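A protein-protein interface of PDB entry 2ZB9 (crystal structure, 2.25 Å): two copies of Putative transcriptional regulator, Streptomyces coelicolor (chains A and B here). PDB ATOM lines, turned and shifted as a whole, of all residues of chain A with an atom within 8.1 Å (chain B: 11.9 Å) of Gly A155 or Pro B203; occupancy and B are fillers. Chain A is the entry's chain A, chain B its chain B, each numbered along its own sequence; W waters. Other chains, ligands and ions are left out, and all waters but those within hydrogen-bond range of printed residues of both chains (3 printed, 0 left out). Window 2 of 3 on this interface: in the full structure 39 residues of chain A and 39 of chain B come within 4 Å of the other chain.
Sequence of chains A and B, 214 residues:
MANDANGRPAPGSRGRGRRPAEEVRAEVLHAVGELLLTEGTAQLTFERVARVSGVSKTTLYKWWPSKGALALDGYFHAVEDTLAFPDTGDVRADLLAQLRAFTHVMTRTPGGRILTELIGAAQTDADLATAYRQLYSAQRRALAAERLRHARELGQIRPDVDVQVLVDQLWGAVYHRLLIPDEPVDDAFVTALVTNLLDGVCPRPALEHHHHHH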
ATOM      1  N   VAL A  91     -27.209  32.477   3.436  1.00  0.00           N
ATOM      2  CA  VAL A  91     -27.863  31.179   3.528  1.00  0.00           C
ATOM      3  C   VAL A  91     -28.941  31.080   4.605  1.00  0.00           C
ATOM      4  O   VAL A  91     -29.946  30.408   4.404  1.00  0.00           O
ATOM      5  CB  VAL A  91     -26.827  30.039   3.714  1.00  0.00           C
ATOM      6  CG1 VAL A  91     -26.142  30.152   5.072  1.00  0.00           C
ATOM      7  CG2 VAL A  91     -27.513  28.689   3.549  1.00  0.00           C
ATOM      8  N   LEU A 148     -27.470  24.780  -1.104  1.00  0.00           N
ATOM      9  CA  LEU A 148     -26.618  24.445   0.037  1.00  0.00           C
ATOM     10  C   LEU A 148     -25.134  24.362  -0.337  1.00  0.00           C
ATOM     11  O   LEU A 148     -24.276  24.873   0.388  1.00  0.00           O
ATOM     12  CB  LEU A 148     -27.090  23.123   0.658  1.00  0.00           C
ATOM     13  CG  LEU A 148     -28.108  23.189   1.807  1.00  0.00           C
ATOM     14  CD1 LEU A 148     -28.933  24.456   1.735  1.00  0.00           C
ATOM     15  CD2 LEU A 148     -28.992  21.953   1.777  1.00  0.00           C
ATOM     16  N   ARG A 149     -24.827  23.720  -1.460  1.00  0.00           N
ATOM     17  CA  ARG A 149     -23.439  23.623  -1.896  1.00  0.00           C
ATOM     18  C   ARG A 149     -22.888  25.010  -2.210  1.00  0.00           C
ATOM     19  O   ARG A 149     -21.705  25.284  -1.982  1.00  0.00           O
ATOM     20  CB  ARG A 149     -23.298  22.740  -3.143  1.00  0.00           C
ATOM     21  CG  ARG A 149     -23.365  21.241  -2.884  1.00  0.00           C
ATOM     22  CD  ARG A 149     -22.722  20.483  -4.044  1.00  0.00           C
ATOM     23  NE  ARG A 149     -23.384  20.764  -5.318  1.00  0.00           N
ATOM     24  CZ  ARG A 149     -24.527  20.202  -5.706  1.00  0.00           C
ATOM     25  NH1 ARG A 149     -25.133  19.320  -4.921  1.00  0.00           N
ATOM     26  NH2 ARG A 149     -25.068  20.524  -6.875  1.00  0.00           N
ATOM     27  N   HIS A 150     -23.736  25.886  -2.741  1.00  0.00           N
ATOM     28  CA  HIS A 150     -23.297  27.240  -3.062  1.00  0.00           C
ATOM     29  C   HIS A 150     -22.867  27.933  -1.770  1.00  0.00           C
ATOM     30  O   HIS A 150     -21.820  28.568  -1.721  1.00  0.00           O
ATOM     31  CB  HIS A 150     -24.417  28.031  -3.751  1.00  0.00           C
ATOM     32  CG  HIS A 150     -23.986  29.376  -4.250  1.00  0.00           C
ATOM     33  ND1 HIS A 150     -22.832  29.567  -4.982  1.00  0.00           N
ATOM     34  CD2 HIS A 150     -24.561  30.596  -4.135  1.00  0.00           C
ATOM     35  CE1 HIS A 150     -22.717  30.845  -5.296  1.00  0.00           C
ATOM     36  NE2 HIS A 150     -23.754  31.490  -4.794  1.00  0.00           N
ATOM     37  N   ALA A 151     -23.670  27.795  -0.721  1.00  0.00           N
ATOM     38  CA  ALA A 151     -23.335  28.392   0.567  1.00  0.00           C
ATOM     39  C   ALA A 151     -22.023  27.791   1.065  1.00  0.00           C
ATOM     40  O   ALA A 151     -21.182  28.496   1.618  1.00  0.00           O
ATOM     41  CB  ALA A 151     -24.448  28.124   1.576  1.00  0.00           C
ATOM     42  N   ARG A 152     -21.838  26.491   0.857  1.00  0.00           N
ATOM     43  CA  ARG A 152     -20.609  25.840   1.302  1.00  0.00           C
ATOM     44  C   ARG A 152     -19.394  26.372   0.538  1.00  0.00           C
ATOM     45  O   ARG A 152     -18.329  26.590   1.126  1.00  0.00           O
ATOM     46  CB  ARG A 152     -20.717  24.321   1.133  1.00  0.00           C
ATOM     47  CG  ARG A 152     -19.537  23.544   1.726  1.00  0.00           C
ATOM     48  CD  ARG A 152     -19.736  22.037   1.596  1.00  0.00           C
ATOM     49  NE  ARG A 152     -19.749  21.625   0.197  1.00  0.00           N
ATOM     50  CZ  ARG A 152     -20.182  20.448  -0.239  1.00  0.00           C
ATOM     51  NH1 ARG A 152     -20.638  19.543   0.621  1.00  0.00           N
ATOM     52  NH2 ARG A 152     -20.187  20.187  -1.540  1.00  0.00           N
ATOM     53  N   GLU A 153     -19.561  26.588  -0.767  1.00  0.00           N
ATOM     54  CA  GLU A 153     -18.479  27.103  -1.604  1.00  0.00           C
ATOM     55  C   GLU A 153     -18.109  28.515  -1.165  1.00  0.00           C
ATOM     56  O   GLU A 153     -16.947  28.913  -1.260  1.00  0.00           O
ATOM     57  CB  GLU A 153     -18.893  27.098  -3.086  1.00  0.00           C
ATOM     58  CG  GLU A 153     -19.129  25.694  -3.641  1.00  0.00           C
ATOM     59  CD  GLU A 153     -19.736  25.670  -5.044  1.00  0.00           C
ATOM     60  OE1 GLU A 153     -19.967  24.550  -5.563  1.00  0.00           O
ATOM     61  OE2 GLU A 153     -19.984  26.754  -5.629  1.00  0.00           O
ATOM     62  N   LEU A 154     -19.091  29.268  -0.674  1.00  0.00           N
ATOM     63  CA  LEU A 154     -18.841  30.632  -0.211  1.00  0.00           C
ATOM     64  C   LEU A 154     -18.360  30.632   1.241  1.00  0.00           C
ATOM     65  O   LEU A 154     -18.105  31.688   1.821  1.00  0.00           O
ATOM     66  CB  LEU A 154     -20.106  31.490  -0.321  1.00  0.00           C
ATOM     67  CG  LEU A 154     -20.733  31.700  -1.703  1.00  0.00           C
ATOM     68  CD1 LEU A 154     -21.848  32.741  -1.603  1.00  0.00           C
ATOM     69  CD2 LEU A 154     -19.669  32.168  -2.692  1.00  0.00           C
ATOM     70  N   GLY A 155     -18.256  29.443   1.830  1.00  0.00           N
ATOM     71  CA  GLY A 155     -17.787  29.321   3.200  1.00  0.00           C
ATOM     72  C   GLY A 155     -18.800  29.506   4.318  1.00  0.00           C
ATOM     73  O   GLY A 155     -18.408  29.622   5.474  1.00  0.00           O
ATOM     74  N   GLN A 156     -20.093  29.517   4.003  1.00  0.00           N
ATOM     75  CA  GLN A 156     -21.111  29.708   5.038  1.00  0.00           C
ATOM     76  C   GLN A 156     -21.526  28.394   5.692  1.00  0.00           C
ATOM     77  O   GLN A 156     -22.276  28.374   6.660  1.00  0.00           O
ATOM     78  CB  GLN A 156     -22.334  30.410   4.447  1.00  0.00           C
ATOM     79  CG  GLN A 156     -21.969  31.567   3.535  1.00  0.00           C
ATOM     80  CD  GLN A 156     -23.141  32.479   3.227  1.00  0.00           C
ATOM     81  OE1 GLN A 156     -24.256  32.020   2.979  1.00  0.00           O
ATOM     82  NE2 GLN A 156     -22.886  33.783   3.226  1.00  0.00           N
ATOM     83  N   ILE A 157     -21.031  27.297   5.142  1.00  0.00           N
ATOM     84  CA  ILE A 157     -21.308  25.965   5.651  1.00  0.00           C
ATOM     85  C   ILE A 157     -19.957  25.260   5.660  1.00  0.00           C
ATOM     86  O   ILE A 157     -19.190  25.392   4.709  1.00  0.00           O
ATOM     87  CB  ILE A 157     -22.302  25.206   4.719  1.00  0.00           C
ATOM     88  CG1 ILE A 157     -23.710  25.797   4.880  1.00  0.00           C
ATOM     89  CG2 ILE A 157     -22.301  23.702   5.043  1.00  0.00           C
ATOM     90  CD1 ILE A 157     -24.763  25.153   3.985  1.00  0.00           C
ATOM     91  N   ARG A 158     -19.653  24.534   6.732  1.00  0.00           N
ATOM     92  CA  ARG A 158     -18.371  23.837   6.815  1.00  0.00           C
ATOM     93  C   ARG A 158     -18.176  23.008   5.555  1.00  0.00           C
ATOM     94  O   ARG A 158     -19.114  22.402   5.047  1.00  0.00           O
ATOM     95  CB  ARG A 158     -18.309  22.968   8.083  1.00  0.00           C
ATOM     96  CG  ARG A 158     -18.337  23.810   9.359  1.00  0.00           C
ATOM     97  CD  ARG A 158     -18.064  23.016  10.638  1.00  0.00           C
ATOM     98  NE  ARG A 158     -19.168  22.142  11.036  1.00  0.00           N
ATOM     99  CZ  ARG A 158     -19.243  20.850  10.739  1.00  0.00           C
ATOM    100  NH1 ARG A 158     -18.278  20.272  10.036  1.00  0.00           N
ATOM    101  NH2 ARG A 158     -20.274  20.127  11.162  1.00  0.00           N
ATOM    102  N   PRO A 159     -16.947  22.984   5.022  1.00  0.00           N
ATOM    103  CA  PRO A 159     -16.655  22.226   3.800  1.00  0.00           C
ATOM    104  C   PRO A 159     -16.820  20.709   3.866  1.00  0.00           C
ATOM    105  O   PRO A 159     -17.000  20.060   2.837  1.00  0.00           O
ATOM    106  CB  PRO A 159     -15.229  22.664   3.454  1.00  0.00           C
ATOM    107  CG  PRO A 159     -14.637  23.000   4.788  1.00  0.00           C
ATOM    108  CD  PRO A 159     -15.756  23.703   5.508  1.00  0.00           C
ATOM    109  N   VAL A 161     -19.333  19.154   5.296  1.00  0.00           N
ATOM    110  CA  VAL A 161     -20.725  18.815   5.540  1.00  0.00           C
ATOM    111  C   VAL A 161     -21.382  18.271   4.277  1.00  0.00           C
ATOM    112  O   VAL A 161     -21.214  18.815   3.184  1.00  0.00           O
ATOM    113  CB  VAL A 161     -21.513  20.049   6.062  1.00  0.00           C
ATOM    114  CG1 VAL A 161     -23.009  19.779   6.039  1.00  0.00           C
ATOM    115  CG2 VAL A 161     -21.076  20.372   7.488  1.00  0.00           C
ATOM    116  N   LEU A 198     -27.822  25.415  11.714  1.00  0.00           N
ATOM    117  CA  LEU A 198     -26.780  26.401  11.490  1.00  0.00           C
ATOM    118  C   LEU A 198     -25.973  26.714  12.744  1.00  0.00           C
ATOM    119  O   LEU A 198     -24.745  26.763  12.695  1.00  0.00           O
ATOM    120  CB  LEU A 198     -27.398  27.693  10.929  1.00  0.00           C
ATOM    121  CG  LEU A 198     -27.468  27.913   9.404  1.00  0.00           C
ATOM    122  CD1 LEU A 198     -27.784  26.628   8.680  1.00  0.00           C
ATOM    123  CD2 LEU A 198     -28.510  28.975   9.100  1.00  0.00           C
ATOM    124  N   ASP A 199     -26.656  26.906  13.869  1.00  0.00           N
ATOM    125  CA  ASP A 199     -25.978  27.249  15.116  1.00  0.00           C
ATOM    126  C   ASP A 199     -25.594  26.066  16.009  1.00  0.00           C
ATOM    127  O   ASP A 199     -24.752  26.204  16.900  1.00  0.00           O
ATOM    128  CB  ASP A 199     -26.833  28.240  15.924  1.00  0.00           C
ATOM    129  CG  ASP A 199     -27.199  29.494  15.125  1.00  0.00           C
ATOM    130  OD1 ASP A 199     -26.333  30.008  14.392  1.00  0.00           O
ATOM    131  OD2 ASP A 199     -28.347  29.975  15.237  1.00  0.00           O
ATOM    132  N   THR B 195     -24.065  14.592  14.338  1.00  0.00           N
ATOM    133  CA  THR B 195     -22.975  15.550  14.335  1.00  0.00           C
ATOM    134  C   THR B 195     -23.393  16.919  13.797  1.00  0.00           C
ATOM    135  O   THR B 195     -23.012  17.954  14.363  1.00  0.00           O
ATOM    136  CB  THR B 195     -21.778  15.008  13.531  1.00  0.00           C
ATOM    137  OG1 THR B 195     -22.166  14.809  12.166  1.00  0.00           O
ATOM    138  CG2 THR B 195     -21.316  13.673  14.119  1.00  0.00           C
ATOM    139  N   ASN B 196     -24.169  16.934  12.711  1.00  0.00           N
ATOM    140  CA  ASN B 196     -24.624  18.204  12.146  1.00  0.00           C
ATOM    141  C   ASN B 196     -25.391  18.995  13.194  1.00  0.00           C
ATOM    142  O   ASN B 196     -25.196  20.192  13.362  1.00  0.00           O
ATOM    143  CB  ASN B 196     -25.572  17.995  10.960  1.00  0.00           C
ATOM    144  CG  ASN B 196     -24.867  17.522   9.705  1.00  0.00           C
ATOM    145  OD1 ASN B 196     -23.657  17.683   9.551  1.00  0.00           O
ATOM    146  ND2 ASN B 196     -25.634  16.957   8.787  1.00  0.00           N
ATOM    147  N   LEU B 198     -25.558  18.477  16.717  1.00  0.00           N
ATOM    148  CA  LEU B 198     -24.838  18.813  17.941  1.00  0.00           C
ATOM    149  C   LEU B 198     -23.782  19.892  17.735  1.00  0.00           C
ATOM    150  O   LEU B 198     -23.667  20.817  18.542  1.00  0.00           O
ATOM    151  CB  LEU B 198     -24.184  17.562  18.540  1.00  0.00           C
ATOM    152  CG  LEU B 198     -25.132  16.459  19.031  1.00  0.00           C
ATOM    153  CD1 LEU B 198     -24.329  15.324  19.642  1.00  0.00           C
ATOM    154  CD2 LEU B 198     -26.091  17.028  20.062  1.00  0.00           C
ATOM    155  N   ASP B 199     -23.018  19.781  16.652  1.00  0.00           N
ATOM    156  CA  ASP B 199     -21.965  20.747  16.368  1.00  0.00           C
ATOM    157  C   ASP B 199     -22.371  21.889  15.426  1.00  0.00           C
ATOM    158  O   ASP B 199     -21.659  22.893  15.324  1.00  0.00           O
ATOM    159  CB  ASP B 199     -20.743  20.027  15.790  1.00  0.00           C
ATOM    160  CG  ASP B 199     -20.274  18.879  16.669  1.00  0.00           C
ATOM    161  OD1 ASP B 199     -20.319  19.019  17.907  1.00  0.00           O
ATOM    162  OD2 ASP B 199     -19.851  17.838  16.125  1.00  0.00           O
ATOM    163  N   GLY B 200     -23.502  21.745  14.742  1.00  0.00           N
ATOM    164  CA  GLY B 200     -23.929  22.782  13.816  1.00  0.00           C
ATOM    165  C   GLY B 200     -23.149  22.663  12.520  1.00  0.00           C
ATOM    166  O   GLY B 200     -22.050  22.110  12.507  1.00  0.00           O
ATOM    167  N   VAL B 201     -23.699  23.184  11.430  1.00  0.00           N
ATOM    168  CA  VAL B 201     -23.030  23.085  10.137  1.00  0.00           C
ATOM    169  C   VAL B 201     -22.315  24.354   9.659  1.00  0.00           C
ATOM    170  O   VAL B 201     -21.785  24.388   8.547  1.00  0.00           O
ATOM    171  CB  VAL B 201     -24.021  22.620   9.047  1.00  0.00           C
ATOM    172  CG1 VAL B 201     -24.655  21.295   9.463  1.00  0.00           C
ATOM    173  CG2 VAL B 201     -25.093  23.675   8.820  1.00  0.00           C
ATOM    174  N   CYS B 202     -22.285  25.387  10.494  1.00  0.00           N
ATOM    175  CA  CYS B 202     -21.605  26.627  10.122  1.00  0.00           C
ATOM    176  C   CYS B 202     -20.246  26.761  10.795  1.00  0.00           C
ATOM    177  O   CYS B 202     -20.020  26.201  11.862  1.00  0.00           O
ATOM    178  CB  CYS B 202     -22.466  27.836  10.476  1.00  0.00           C
ATOM    179  SG  CYS B 202     -23.968  27.923   9.500  1.00  0.00           S
ATOM    180  N   PRO B 203     -19.323  27.508  10.170  1.00  0.00           N
ATOM    181  CA  PRO B 203     -17.975  27.712  10.714  1.00  0.00           C
ATOM    182  C   PRO B 203     -18.005  28.375  12.090  1.00  0.00           C
ATOM    183  O   PRO B 203     -18.932  29.168  12.344  1.00  0.00           O
ATOM    184  CB  PRO B 203     -17.312  28.607   9.665  1.00  0.00           C
ATOM    185  CG  PRO B 203     -18.018  28.229   8.397  1.00  0.00           C
ATOM    186  CD  PRO B 203     -19.454  28.145   8.848  1.00  0.00           C
HETATM  187  O   HOH W   1     -21.729  25.702  16.967  1.00  0.00           O
HETATM  188  O   HOH W   2     -21.419  17.544  10.847  1.00  0.00           O
HETATM  189  O   HOH W   3     -22.169  26.570  13.787  1.00  0.00           O
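O of Gln A156 is in hydrogen-bond range of SG of Cys B202 (3.3 Å).
NH2 of Arg A158 lies within hydrogen-bond range of O of Gly B200 (3.0 Å).
O of Val B201 lies within hydrogen-bond range of N of Arg A158 (2.8 Å).
O of Leu A198 lies close to SG of Cys B202 (3.5 Å).
N of Val A91 lies within hydrogen-bond range of OE1 of Gln A156 (3.0 Å).
The backbone NH (N) of Gln A156 is in hydrogen-bond range of the backbone carbonyl oxygen (O) of Ala A151, 2.8 Å away.
Among the printed residues, pairs that only touch across the chains: Gly A155 with Pro B203 (3.3 Å), Gln A156 with Pro B203 (3.6 Å), Ile A157 with Val B201 (3.3 Å), Arg A158 with Cys B202 (3.8 Å), Arg A158 with Pro B203 (3.9 Å) and Leu A198 with Val B201 (3.9 Å).
Printed residues of chain B within 4 Å of Gln A156: Cys B202 (3.3 Å) and Pro B203 (3.6 Å).
Of chain B, only Gly B200, Val B201, Cys B202 and Pro B203 come within 4 Å of Arg A158.
Of the printed residues of chain B, Leu A198 touches Val B201 and Cys B202.
Of the printed residues of chain A, Val B201 touches Ile A157, Arg A158 and Leu A198.
Of the printed residues of chain A, Cys B202 touches Gln A156 (3.3 Å), Arg A158 (3.8 Å) and Leu A198 (3.4 Å).
Of the printed residues of chain A, Pro B203 touches Gly A155, Gln A156 and Arg A158.
The nearest printed residue of chain B that does not touch Leu A198 is Gly B200 (4.2 Å).
Of the 8 printed residues of chain B, 4 touch a printed residue of chain A.
Printed residues of chain B that touch a printed residue of chain A: Gly B200, Val B201, Cys B202 and Pro B203.
Along chain B the printed residues that touch a printed residue of chain A span positions 200 to 203.
Of the 16 printed residues of chain A, 5 touch a printed residue of chain B.
Among the printed residues, 10 pairs touch across the chains.
Among the printed residues, no Asp or Glu carboxylate lies within 4 Å of a Lys or Arg side-chain nitrogen of the other chain.
2 positions are printed for both chains.
Water W2 lies within hydrogen-bond range of OD1 of Asn B196 (2.6 Å), NH2 of Arg A158 (2.8 Å) and OG1 of Thr B195 (3.1 Å).
Water W3 bridges the backbone carbonyl oxygen (O) of Leu A198 (2.8 Å) and the backbone carbonyl oxygen (O) of Cys B202 (2.9 Å).
Water W1 lies within hydrogen-bond range of the backbone carbonyl oxygen of Asp A199 (3.1 Å) and the backbone carbonyl oxygen of Asp B199 (3.3 Å).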
